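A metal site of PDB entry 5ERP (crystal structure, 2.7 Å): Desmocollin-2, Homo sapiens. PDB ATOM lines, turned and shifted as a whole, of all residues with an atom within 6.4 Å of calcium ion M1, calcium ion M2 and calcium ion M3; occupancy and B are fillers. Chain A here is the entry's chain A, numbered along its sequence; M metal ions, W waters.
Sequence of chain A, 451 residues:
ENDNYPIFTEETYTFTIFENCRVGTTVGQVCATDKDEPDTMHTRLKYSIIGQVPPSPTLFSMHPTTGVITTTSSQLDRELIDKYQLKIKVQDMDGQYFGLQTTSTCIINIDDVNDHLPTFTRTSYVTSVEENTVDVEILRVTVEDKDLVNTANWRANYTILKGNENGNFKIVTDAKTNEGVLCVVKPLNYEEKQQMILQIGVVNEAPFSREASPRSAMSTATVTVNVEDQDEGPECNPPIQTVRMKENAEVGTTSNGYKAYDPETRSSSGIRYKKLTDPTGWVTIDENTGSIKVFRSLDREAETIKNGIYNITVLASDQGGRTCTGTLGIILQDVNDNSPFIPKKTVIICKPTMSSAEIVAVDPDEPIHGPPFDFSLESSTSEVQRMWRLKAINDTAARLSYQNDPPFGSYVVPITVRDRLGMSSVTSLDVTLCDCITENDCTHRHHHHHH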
ATOM      1  N   GLU A  19      10.737 -13.192  -4.374  1.00  0.00           N
ATOM      2  CA  GLU A  19      10.388 -11.882  -3.840  1.00  0.00           C
ATOM      3  C   GLU A  19       9.124 -11.359  -4.523  1.00  0.00           C
ATOM      4  O   GLU A  19       8.770 -11.814  -5.619  1.00  0.00           O
ATOM      5  CB  GLU A  19      11.545 -10.899  -4.025  1.00  0.00           C
ATOM      6  CG  GLU A  19      11.918 -10.668  -5.483  1.00  0.00           C
ATOM      7  CD  GLU A  19      13.030  -9.648  -5.638  1.00  0.00           C
ATOM      8  OE1 GLU A  19      13.085  -8.679  -4.846  1.00  0.00           O
ATOM      9  OE2 GLU A  19      13.851  -9.817  -6.555  1.00  0.00           O
ATOM     10  N   ASN A  20       8.471 -10.404  -3.879  1.00  0.00           N
ATOM     11  CA  ASN A  20       7.258  -9.791  -4.407  1.00  0.00           C
ATOM     12  C   ASN A  20       6.104 -10.781  -4.578  1.00  0.00           C
ATOM     13  O   ASN A  20       5.118 -10.478  -5.254  1.00  0.00           O
ATOM     14  CB  ASN A  20       7.540  -9.100  -5.739  1.00  0.00           C
ATOM     15  CG  ASN A  20       8.725  -8.167  -5.675  1.00  0.00           C
ATOM     16  OD1 ASN A  20       9.055  -7.659  -4.599  1.00  0.00           O
ATOM     17  ND2 ASN A  20       9.359  -7.918  -6.817  1.00  0.00           N
ATOM     18  N   LEU A  76       8.370  -8.718   0.579  1.00  0.00           N
ATOM     19  CA  LEU A  76       9.637  -9.437   0.599  1.00  0.00           C
ATOM     20  C   LEU A  76      10.522  -8.893  -0.522  1.00  0.00           C
ATOM     21  O   LEU A  76      10.131  -8.910  -1.686  1.00  0.00           O
ATOM     22  CB  LEU A  76       9.402 -10.935   0.424  1.00  0.00           C
ATOM     23  CG  LEU A  76       8.598 -11.609   1.534  1.00  0.00           C
ATOM     24  CD1 LEU A  76       7.807 -12.783   0.976  1.00  0.00           C
ATOM     25  CD2 LEU A  76       9.522 -12.042   2.667  1.00  0.00           C
ATOM     26  N   ASP A  77      11.709  -8.428  -0.153  1.00  0.00           N
ATOM     27  CA  ASP A  77      12.597  -7.761  -1.098  1.00  0.00           C
ATOM     28  C   ASP A  77      14.019  -8.289  -0.979  1.00  0.00           C
ATOM     29  O   ASP A  77      14.689  -8.069   0.036  1.00  0.00           O
ATOM     30  CB  ASP A  77      12.567  -6.250  -0.877  1.00  0.00           C
ATOM     31  CG  ASP A  77      13.212  -5.476  -2.016  1.00  0.00           C
ATOM     32  OD1 ASP A  77      13.516  -6.080  -3.057  1.00  0.00           O
ATOM     33  OD2 ASP A  77      13.410  -4.251  -1.866  1.00  0.00           O
ATOM     34  N   ARG A  78      14.469  -8.981  -2.013  1.00  0.00           N
ATOM     35  CA  ARG A  78      15.767  -9.638  -2.016  1.00  0.00           C
ATOM     36  C   ARG A  78      16.902  -8.627  -1.868  1.00  0.00           C
ATOM     37  O   ARG A  78      17.932  -8.926  -1.264  1.00  0.00           O
ATOM     38  CB  ARG A  78      15.949 -10.439  -3.318  1.00  0.00           C
ATOM     39  CG  ARG A  78      16.987 -11.552  -3.213  1.00  0.00           C
ATOM     40  CD  ARG A  78      17.772 -11.778  -4.508  1.00  0.00           C
ATOM     41  NE  ARG A  78      19.107 -11.201  -4.439  1.00  0.00           N
ATOM     42  CZ  ARG A  78      19.489 -10.062  -5.016  1.00  0.00           C
ATOM     43  NH1 ARG A  78      18.642  -9.356  -5.753  1.00  0.00           N
ATOM     44  NH2 ARG A  78      20.734  -9.654  -4.853  1.00  0.00           N
ATOM     45  N   GLU A  79      16.705  -7.431  -2.416  1.00  0.00           N
ATOM     46  CA  GLU A  79      17.730  -6.389  -2.403  1.00  0.00           C
ATOM     47  C   GLU A  79      17.855  -5.701  -1.043  1.00  0.00           C
ATOM     48  O   GLU A  79      18.787  -4.941  -0.811  1.00  0.00           O
ATOM     49  CB  GLU A  79      17.441  -5.358  -3.499  1.00  0.00           C
ATOM     50  CG  GLU A  79      17.742  -5.858  -4.915  1.00  0.00           C
ATOM     51  CD  GLU A  79      16.658  -6.762  -5.480  1.00  0.00           C
ATOM     52  OE1 GLU A  79      15.517  -6.732  -4.970  1.00  0.00           O
ATOM     53  OE2 GLU A  79      16.952  -7.512  -6.438  1.00  0.00           O
ATOM     54  N   LEU A  80      16.893  -5.963  -0.152  1.00  0.00           N
ATOM     55  CA  LEU A  80      16.952  -5.430   1.220  1.00  0.00           C
ATOM     56  C   LEU A  80      17.339  -6.540   2.193  1.00  0.00           C
ATOM     57  O   LEU A  80      18.264  -6.378   2.987  1.00  0.00           O
ATOM     58  CB  LEU A  80      15.611  -4.819   1.622  1.00  0.00           C
ATOM     59  CG  LEU A  80      15.185  -3.544   0.874  1.00  0.00           C
ATOM     60  CD1 LEU A  80      13.763  -3.151   1.245  1.00  0.00           C
ATOM     61  CD2 LEU A  80      16.145  -2.402   1.178  1.00  0.00           C
ATOM     62  N   ASP A 111      14.465 -15.787  -3.520  1.00  0.00           N
ATOM     63  CA  ASP A 111      14.977 -15.914  -4.865  1.00  0.00           C
ATOM     64  C   ASP A 111      14.771 -14.599  -5.600  1.00  0.00           C
ATOM     65  O   ASP A 111      13.931 -13.783  -5.210  1.00  0.00           O
ATOM     66  CB  ASP A 111      14.279 -17.059  -5.595  1.00  0.00           C
ATOM     67  CG  ASP A 111      15.185 -17.785  -6.568  1.00  0.00           C
ATOM     68  OD1 ASP A 111      16.091 -17.143  -7.141  1.00  0.00           O
ATOM     69  OD2 ASP A 111      14.986 -18.995  -6.764  1.00  0.00           O
ATOM     70  N   ASP A 112      15.530 -14.382  -6.673  1.00  0.00           N
ATOM     71  CA  ASP A 112      15.514 -13.113  -7.379  1.00  0.00           C
ATOM     72  C   ASP A 112      14.527 -13.113  -8.553  1.00  0.00           C
ATOM     73  O   ASP A 112      14.348 -14.126  -9.225  1.00  0.00           O
ATOM     74  CB  ASP A 112      16.916 -12.775  -7.890  1.00  0.00           C
ATOM     75  CG  ASP A 112      17.011 -11.390  -8.500  1.00  0.00           C
ATOM     76  OD1 ASP A 112      16.640 -10.421  -7.807  1.00  0.00           O
ATOM     77  OD2 ASP A 112      17.454 -11.282  -9.664  1.00  0.00           O
ATOM     78  N   VAL A 113      13.887 -11.965  -8.763  1.00  0.00           N
ATOM     79  CA  VAL A 113      13.117 -11.712  -9.981  1.00  0.00           C
ATOM     80  C   VAL A 113      13.619 -10.409 -10.572  1.00  0.00           C
ATOM     81  O   VAL A 113      14.200  -9.583  -9.861  1.00  0.00           O
ATOM     82  CB  VAL A 113      11.587 -11.649  -9.723  1.00  0.00           C
ATOM     83  CG1 VAL A 113      11.116 -12.852  -8.912  1.00  0.00           C
ATOM     84  CG2 VAL A 113      11.207 -10.355  -9.022  1.00  0.00           C
ATOM     85  N   ASN A 114      13.409 -10.209 -11.870  1.00  0.00           N
ATOM     86  CA  ASN A 114      13.927  -9.041 -12.565  1.00  0.00           C
ATOM     87  C   ASN A 114      13.049  -7.804 -12.344  1.00  0.00           C
ATOM     88  O   ASN A 114      12.142  -7.543 -13.139  1.00  0.00           O
ATOM     89  CB  ASN A 114      14.054  -9.341 -14.065  1.00  0.00           C
ATOM     90  CG  ASN A 114      14.654  -8.186 -14.855  1.00  0.00           C
ATOM     91  OD1 ASN A 114      15.498  -7.449 -14.358  1.00  0.00           O
ATOM     92  ND2 ASN A 114      14.225  -8.050 -16.096  1.00  0.00           N
ATOM     93  N   ASP A 115      13.311  -7.067 -11.276  1.00  0.00           N
ATOM     94  CA  ASP A 115      12.512  -5.882 -10.940  1.00  0.00           C
ATOM     95  C   ASP A 115      13.345  -4.606 -10.870  1.00  0.00           C
ATOM     96  O   ASP A 115      12.849  -3.563 -10.427  1.00  0.00           O
ATOM     97  CB  ASP A 115      11.765  -6.099  -9.617  1.00  0.00           C
ATOM     98  CG  ASP A 115      12.681  -6.512  -8.477  1.00  0.00           C
ATOM     99  OD1 ASP A 115      13.883  -6.721  -8.708  1.00  0.00           O
ATOM    100  OD2 ASP A 115      12.171  -6.630  -7.351  1.00  0.00           O
ATOM    101  N   HIS A 116      14.600  -4.683 -11.294  1.00  0.00           N
ATOM    102  CA  HIS A 116      15.412  -3.484 -11.557  1.00  0.00           C
ATOM    103  C   HIS A 116      15.877  -3.478 -13.002  1.00  0.00           C
ATOM    104  O   HIS A 116      16.601  -4.370 -13.435  1.00  0.00           O
ATOM    105  CB  HIS A 116      16.627  -3.420 -10.622  1.00  0.00           C
ATOM    106  CG  HIS A 116      16.287  -3.222  -9.181  1.00  0.00           C
ATOM    107  ND1 HIS A 116      16.096  -4.271  -8.306  1.00  0.00           N
ATOM    108  CD2 HIS A 116      16.122  -2.089  -8.455  1.00  0.00           C
ATOM    109  CE1 HIS A 116      15.817  -3.792  -7.110  1.00  0.00           C
ATOM    110  NE2 HIS A 116      15.820  -2.469  -7.171  1.00  0.00           N
ATOM    111  N   LEU A 117      15.470  -2.465 -13.767  1.00  0.00           N
ATOM    112  CA  LEU A 117      15.917  -2.343 -15.146  1.00  0.00           C
ATOM    113  C   LEU A 117      17.351  -1.850 -15.167  1.00  0.00           C
ATOM    114  O   LEU A 117      17.723  -0.992 -14.351  1.00  0.00           O
ATOM    115  CB  LEU A 117      15.023  -1.391 -15.940  1.00  0.00           C
ATOM    116  CG  LEU A 117      13.563  -1.818 -16.068  1.00  0.00           C
ATOM    117  CD1 LEU A 117      12.698  -0.634 -16.467  1.00  0.00           C
ATOM    118  CD2 LEU A 117      13.440  -2.926 -17.115  1.00  0.00           C
ATOM    119  N   PRO A 118      18.182  -2.366 -16.088  1.00  0.00           N
ATOM    120  CA  PRO A 118      19.563  -1.895 -16.125  1.00  0.00           C
ATOM    121  C   PRO A 118      19.642  -0.509 -16.743  1.00  0.00           C
ATOM    122  O   PRO A 118      18.911  -0.200 -17.679  1.00  0.00           O
ATOM    123  CB  PRO A 118      20.264  -2.939 -16.985  1.00  0.00           C
ATOM    124  CG  PRO A 118      19.207  -3.404 -17.926  1.00  0.00           C
ATOM    125  CD  PRO A 118      17.895  -3.310 -17.180  1.00  0.00           C
ATOM    126  N   ASP A 145      22.722  -2.497 -12.312  1.00  0.00           N
ATOM    127  CA  ASP A 145      21.591  -3.400 -12.164  1.00  0.00           C
ATOM    128  C   ASP A 145      21.646  -4.020 -10.776  1.00  0.00           C
ATOM    129  O   ASP A 145      22.610  -4.706 -10.435  1.00  0.00           O
ATOM    130  CB  ASP A 145      21.599  -4.482 -13.242  1.00  0.00           C
ATOM    131  CG  ASP A 145      20.258  -5.179 -13.384  1.00  0.00           C
ATOM    132  OD1 ASP A 145      19.655  -5.534 -12.355  1.00  0.00           O
ATOM    133  OD2 ASP A 145      19.812  -5.369 -14.533  1.00  0.00           O
ATOM    134  N   LYS A 146      20.601  -3.783  -9.993  1.00  0.00           N
ATOM    135  CA  LYS A 146      20.591  -4.194  -8.597  1.00  0.00           C
ATOM    136  C   LYS A 146      20.124  -5.634  -8.407  1.00  0.00           C
ATOM    137  O   LYS A 146      20.097  -6.132  -7.279  1.00  0.00           O
ATOM    138  CB  LYS A 146      19.709  -3.245  -7.793  1.00  0.00           C
ATOM    139  CG  LYS A 146      20.380  -1.916  -7.518  1.00  0.00           C
ATOM    140  CD  LYS A 146      19.393  -0.827  -7.153  1.00  0.00           C
ATOM    141  CE  LYS A 146      20.080   0.511  -6.957  1.00  0.00           C
ATOM    142  NZ  LYS A 146      21.148   0.433  -5.914  1.00  0.00           N
ATOM    143  N   ASP A 147      19.783  -6.304  -9.500  1.00  0.00           N
ATOM    144  CA  ASP A 147      19.329  -7.691  -9.400  1.00  0.00           C
ATOM    145  C   ASP A 147      20.526  -8.607  -9.167  1.00  0.00           C
ATOM    146  O   ASP A 147      21.663  -8.149  -9.102  1.00  0.00           O
ATOM    147  CB  ASP A 147      18.562  -8.102 -10.662  1.00  0.00           C
ATOM    148  CG  ASP A 147      17.229  -7.391 -10.783  1.00  0.00           C
ATOM    149  OD1 ASP A 147      16.586  -7.143  -9.741  1.00  0.00           O
ATOM    150  OD2 ASP A 147      16.814  -7.089 -11.923  1.00  0.00           O
ATOM    151  N   LEU A 148      20.251  -9.894  -9.044  1.00  0.00           N
ATOM    152  CA  LEU A 148      21.255 -10.861  -8.624  1.00  0.00           C
ATOM    153  C   LEU A 148      22.286 -11.154  -9.716  1.00  0.00           C
ATOM    154  O   LEU A 148      21.925 -11.523 -10.833  1.00  0.00           O
ATOM    155  CB  LEU A 148      20.579 -12.150  -8.172  1.00  0.00           C
ATOM    156  CG  LEU A 148      21.495 -13.298  -7.740  1.00  0.00           C
ATOM    157  CD1 LEU A 148      22.365 -12.875  -6.575  1.00  0.00           C
ATOM    158  CD2 LEU A 148      20.665 -14.516  -7.384  1.00  0.00           C
ATOM    159  N   ALA A 152      19.963 -14.094 -15.668  1.00  0.00           N
ATOM    160  CA  ALA A 152      19.276 -13.457 -16.784  1.00  0.00           C
ATOM    161  C   ALA A 152      18.544 -12.181 -16.349  1.00  0.00           C
ATOM    162  O   ALA A 152      18.107 -11.399 -17.193  1.00  0.00           O
ATOM    163  CB  ALA A 152      18.291 -14.432 -17.422  1.00  0.00           C
ATOM    164  N   ASN A 153      18.400 -11.993 -15.047  1.00  0.00           N
ATOM    165  CA  ASN A 153      17.777 -10.788 -14.507  1.00  0.00           C
ATOM    166  C   ASN A 153      18.788  -9.664 -14.367  1.00  0.00           C
ATOM    167  O   ASN A 153      18.424  -8.528 -14.057  1.00  0.00           O
ATOM    168  CB  ASN A 153      17.155 -11.078 -13.146  1.00  0.00           C
ATOM    169  CG  ASN A 153      16.136 -12.190 -13.183  1.00  0.00           C
ATOM    170  OD1 ASN A 153      15.523 -12.460 -14.216  1.00  0.00           O
ATOM    171  ND2 ASN A 153      15.960 -12.871 -12.052  1.00  0.00           N
ATOM    172  N   TRP A 154      20.056  -9.976 -14.604  1.00  0.00           N
ATOM    173  CA  TRP A 154      21.150  -9.044 -14.353  1.00  0.00           C
ATOM    174  C   TRP A 154      21.932  -8.677 -15.607  1.00  0.00           C
ATOM    175  O   TRP A 154      22.106  -7.491 -15.916  1.00  0.00           O
ATOM    176  CB  TRP A 154      22.109  -9.649 -13.328  1.00  0.00           C
ATOM    177  CG  TRP A 154      23.332  -8.839 -13.068  1.00  0.00           C
ATOM    178  CD1 TRP A 154      23.428  -7.719 -12.293  1.00  0.00           C
ATOM    179  CD2 TRP A 154      24.648  -9.091 -13.562  1.00  0.00           C
ATOM    180  NE1 TRP A 154      24.715  -7.261 -12.277  1.00  0.00           N
ATOM    181  CE2 TRP A 154      25.491  -8.080 -13.044  1.00  0.00           C
ATOM    182  CE3 TRP A 154      25.201 -10.076 -14.379  1.00  0.00           C
ATOM    183  CZ2 TRP A 154      26.851  -8.027 -13.332  1.00  0.00           C
ATOM    184  CZ3 TRP A 154      26.552 -10.027 -14.665  1.00  0.00           C
ATOM    185  CH2 TRP A 154      27.359  -9.013 -14.141  1.00  0.00           C
ATOM    186  N   ARG A 155      22.408  -9.682 -16.331  1.00  0.00           N
ATOM    187  CA  ARG A 155      23.327  -9.458 -17.446  1.00  0.00           C
ATOM    188  C   ARG A 155      22.667  -8.716 -18.596  1.00  0.00           C
ATOM    189  O   ARG A 155      21.497  -8.938 -18.907  1.00  0.00           O
ATOM    190  CB  ARG A 155      23.890 -10.786 -17.942  1.00  0.00           C
ATOM    191  CG  ARG A 155      22.874 -11.725 -18.541  1.00  0.00           C
ATOM    192  CD  ARG A 155      23.548 -12.999 -19.040  1.00  0.00           C
ATOM    193  NE  ARG A 155      22.910 -14.208 -18.523  1.00  0.00           N
ATOM    194  CZ  ARG A 155      23.357 -14.920 -17.499  1.00  0.00           C
ATOM    195  NH1 ARG A 155      24.463 -14.566 -16.844  1.00  0.00           N
ATOM    196  NH2 ARG A 155      22.697 -15.999 -17.118  1.00  0.00           N
ATOM    197  N   ASN A 204      17.869  -6.578 -20.064  1.00  0.00           N
ATOM    198  CA  ASN A 204      18.351  -7.870 -19.565  1.00  0.00           C
ATOM    199  C   ASN A 204      17.951  -8.969 -20.541  1.00  0.00           C
ATOM    200  O   ASN A 204      17.139  -8.750 -21.438  1.00  0.00           O
ATOM    201  CB  ASN A 204      17.778  -8.175 -18.187  1.00  0.00           C
ATOM    202  CG  ASN A 204      18.003  -7.049 -17.195  1.00  0.00           C
ATOM    203  OD1 ASN A 204      17.044  -6.453 -16.703  1.00  0.00           O
ATOM    204  ND2 ASN A 204      19.257  -6.764 -16.885  1.00  0.00           N
ATOM    205  N   PHE A 208      11.392  -7.606 -17.875  1.00  0.00           N
ATOM    206  CA  PHE A 208      11.099  -6.946 -16.598  1.00  0.00           C
ATOM    207  C   PHE A 208       9.987  -7.739 -15.894  1.00  0.00           C
ATOM    208  O   PHE A 208       9.235  -8.450 -16.573  1.00  0.00           O
ATOM    209  CB  PHE A 208      10.661  -5.494 -16.844  1.00  0.00           C
ATOM    210  CG  PHE A 208      10.630  -4.626 -15.619  1.00  0.00           C
ATOM    211  CD1 PHE A 208      11.658  -4.674 -14.682  1.00  0.00           C
ATOM    212  CD2 PHE A 208       9.582  -3.749 -15.396  1.00  0.00           C
ATOM    213  CE1 PHE A 208      11.631  -3.856 -13.561  1.00  0.00           C
ATOM    214  CE2 PHE A 208       9.552  -2.944 -14.271  1.00  0.00           C
ATOM    215  CZ  PHE A 208      10.576  -2.997 -13.353  1.00  0.00           C
HETATM  216 CA    CA M   1      15.371  -8.378  -7.931  1.00  0.00          CA
HETATM  217 CA    CA M   2      13.192  -6.251  -5.307  1.00  0.00          CA
HETATM  218 CA    CA M   3      17.629  -6.333 -13.972  1.00  0.00          CA
HETATM  219  O   HOH W   1      13.344  -3.807  -5.466  1.00  0.00           O
HETATM  220  O   HOH W   2      10.951  -6.335  -4.541  1.00  0.00           O
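A ring nitrogen (ND1) of His 116 sits close to the side-chain carboxylate (OD1) of Asp 115 (3.3 Å).
The side-chain carboxylate (OD2) of Asp 115 lies close to the side-chain amide nitrogen (ND2) of Asn 20, 3.1 Å away.
OD2 of Asp 112 lies within hydrogen-bond range of ND2 of Asn 153, at 3.2 Å.
The guanidinium group (NH1) of Arg 78 sits close to the side-chain carboxylate (OE2) of Glu 79 (2.6 Å).
The side-chain carboxylate (OD2) of Asp 112 sits at hydrogen-bond distance from the backbone NH (N) of Leu 148.
The side-chain amide nitrogen of Asn 114 lies close to the backbone NH of Phe 208 (3.4 Å).
OE1 of Glu 19 lies close to N of Arg 78, at 3.2 Å.
O of Trp 154 is in hydrogen-bond range of ND2 of Asn 204.
Four residues have an atom within 4 Å of calcium ion M2: Glu 19, Asp 77, Glu 79 and Asp 115.
The nearest printed residue that does not touch calcium ion M2 is His 116 (4.02 Å).
Six residues have an atom within 4 Å of calcium ion M3: Asn 114, His 116, Asp 145, Asp 147, Asn 153 and Asn 204.
Along chain A the residues within 4 Å of calcium ion M3 span positions 114 to 204.
Calcium ion M1 is bound by the side-chain carboxylate (OE2) of Glu 79 (2.3 Å), the side-chain carboxylate (OD1) of Asp 115 (2.4 Å), the side-chain carboxylate (OD1) of Asp 112 (2.4 Å), the side-chain carboxylate (OE2) of Glu 19 (2.5 Å), the side-chain carboxylate (OD1) of Asp 147 (2.5 Å) and the backbone carbonyl oxygen (O) of Val 113 (2.6 Å).
Calcium ion M2 is bound by the side-chain carboxylate of Asp 77 (2.3 Å), the side-chain carboxylate of Asp 115 (2.3 Å), water W2 (2.4 Å), the side-chain carboxylate of Glu 79 (2.4 Å), water W1 (2.5 Å) and the side-chain carboxylate of Glu 19 (2.5 Å).
Calcium ion M2 has six donor atoms within binding distance.
Calcium ion M3 is bound by O of His 116, 2.3 Å away.
Calcium ion M3 is bound by OD2 of Asp 147 (2.3 Å).
Calcium ion M3 is bound by the backbone carbonyl oxygen (O) of Asn 153, at 2.3 Å.
OD1 of Asn 114 binds calcium ion M3 (2.4 Å).
OD2 of Asp 145 binds calcium ion M3.
OD1 of Asp 145 is bound to calcium ion M3, 2.7 Å away.
Calcium ion M3 is bound by the side-chain amide oxygen (OD1) of Asn 204 (2.8 Å).
Calcium ion M3 has seven donor atoms within binding distance.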
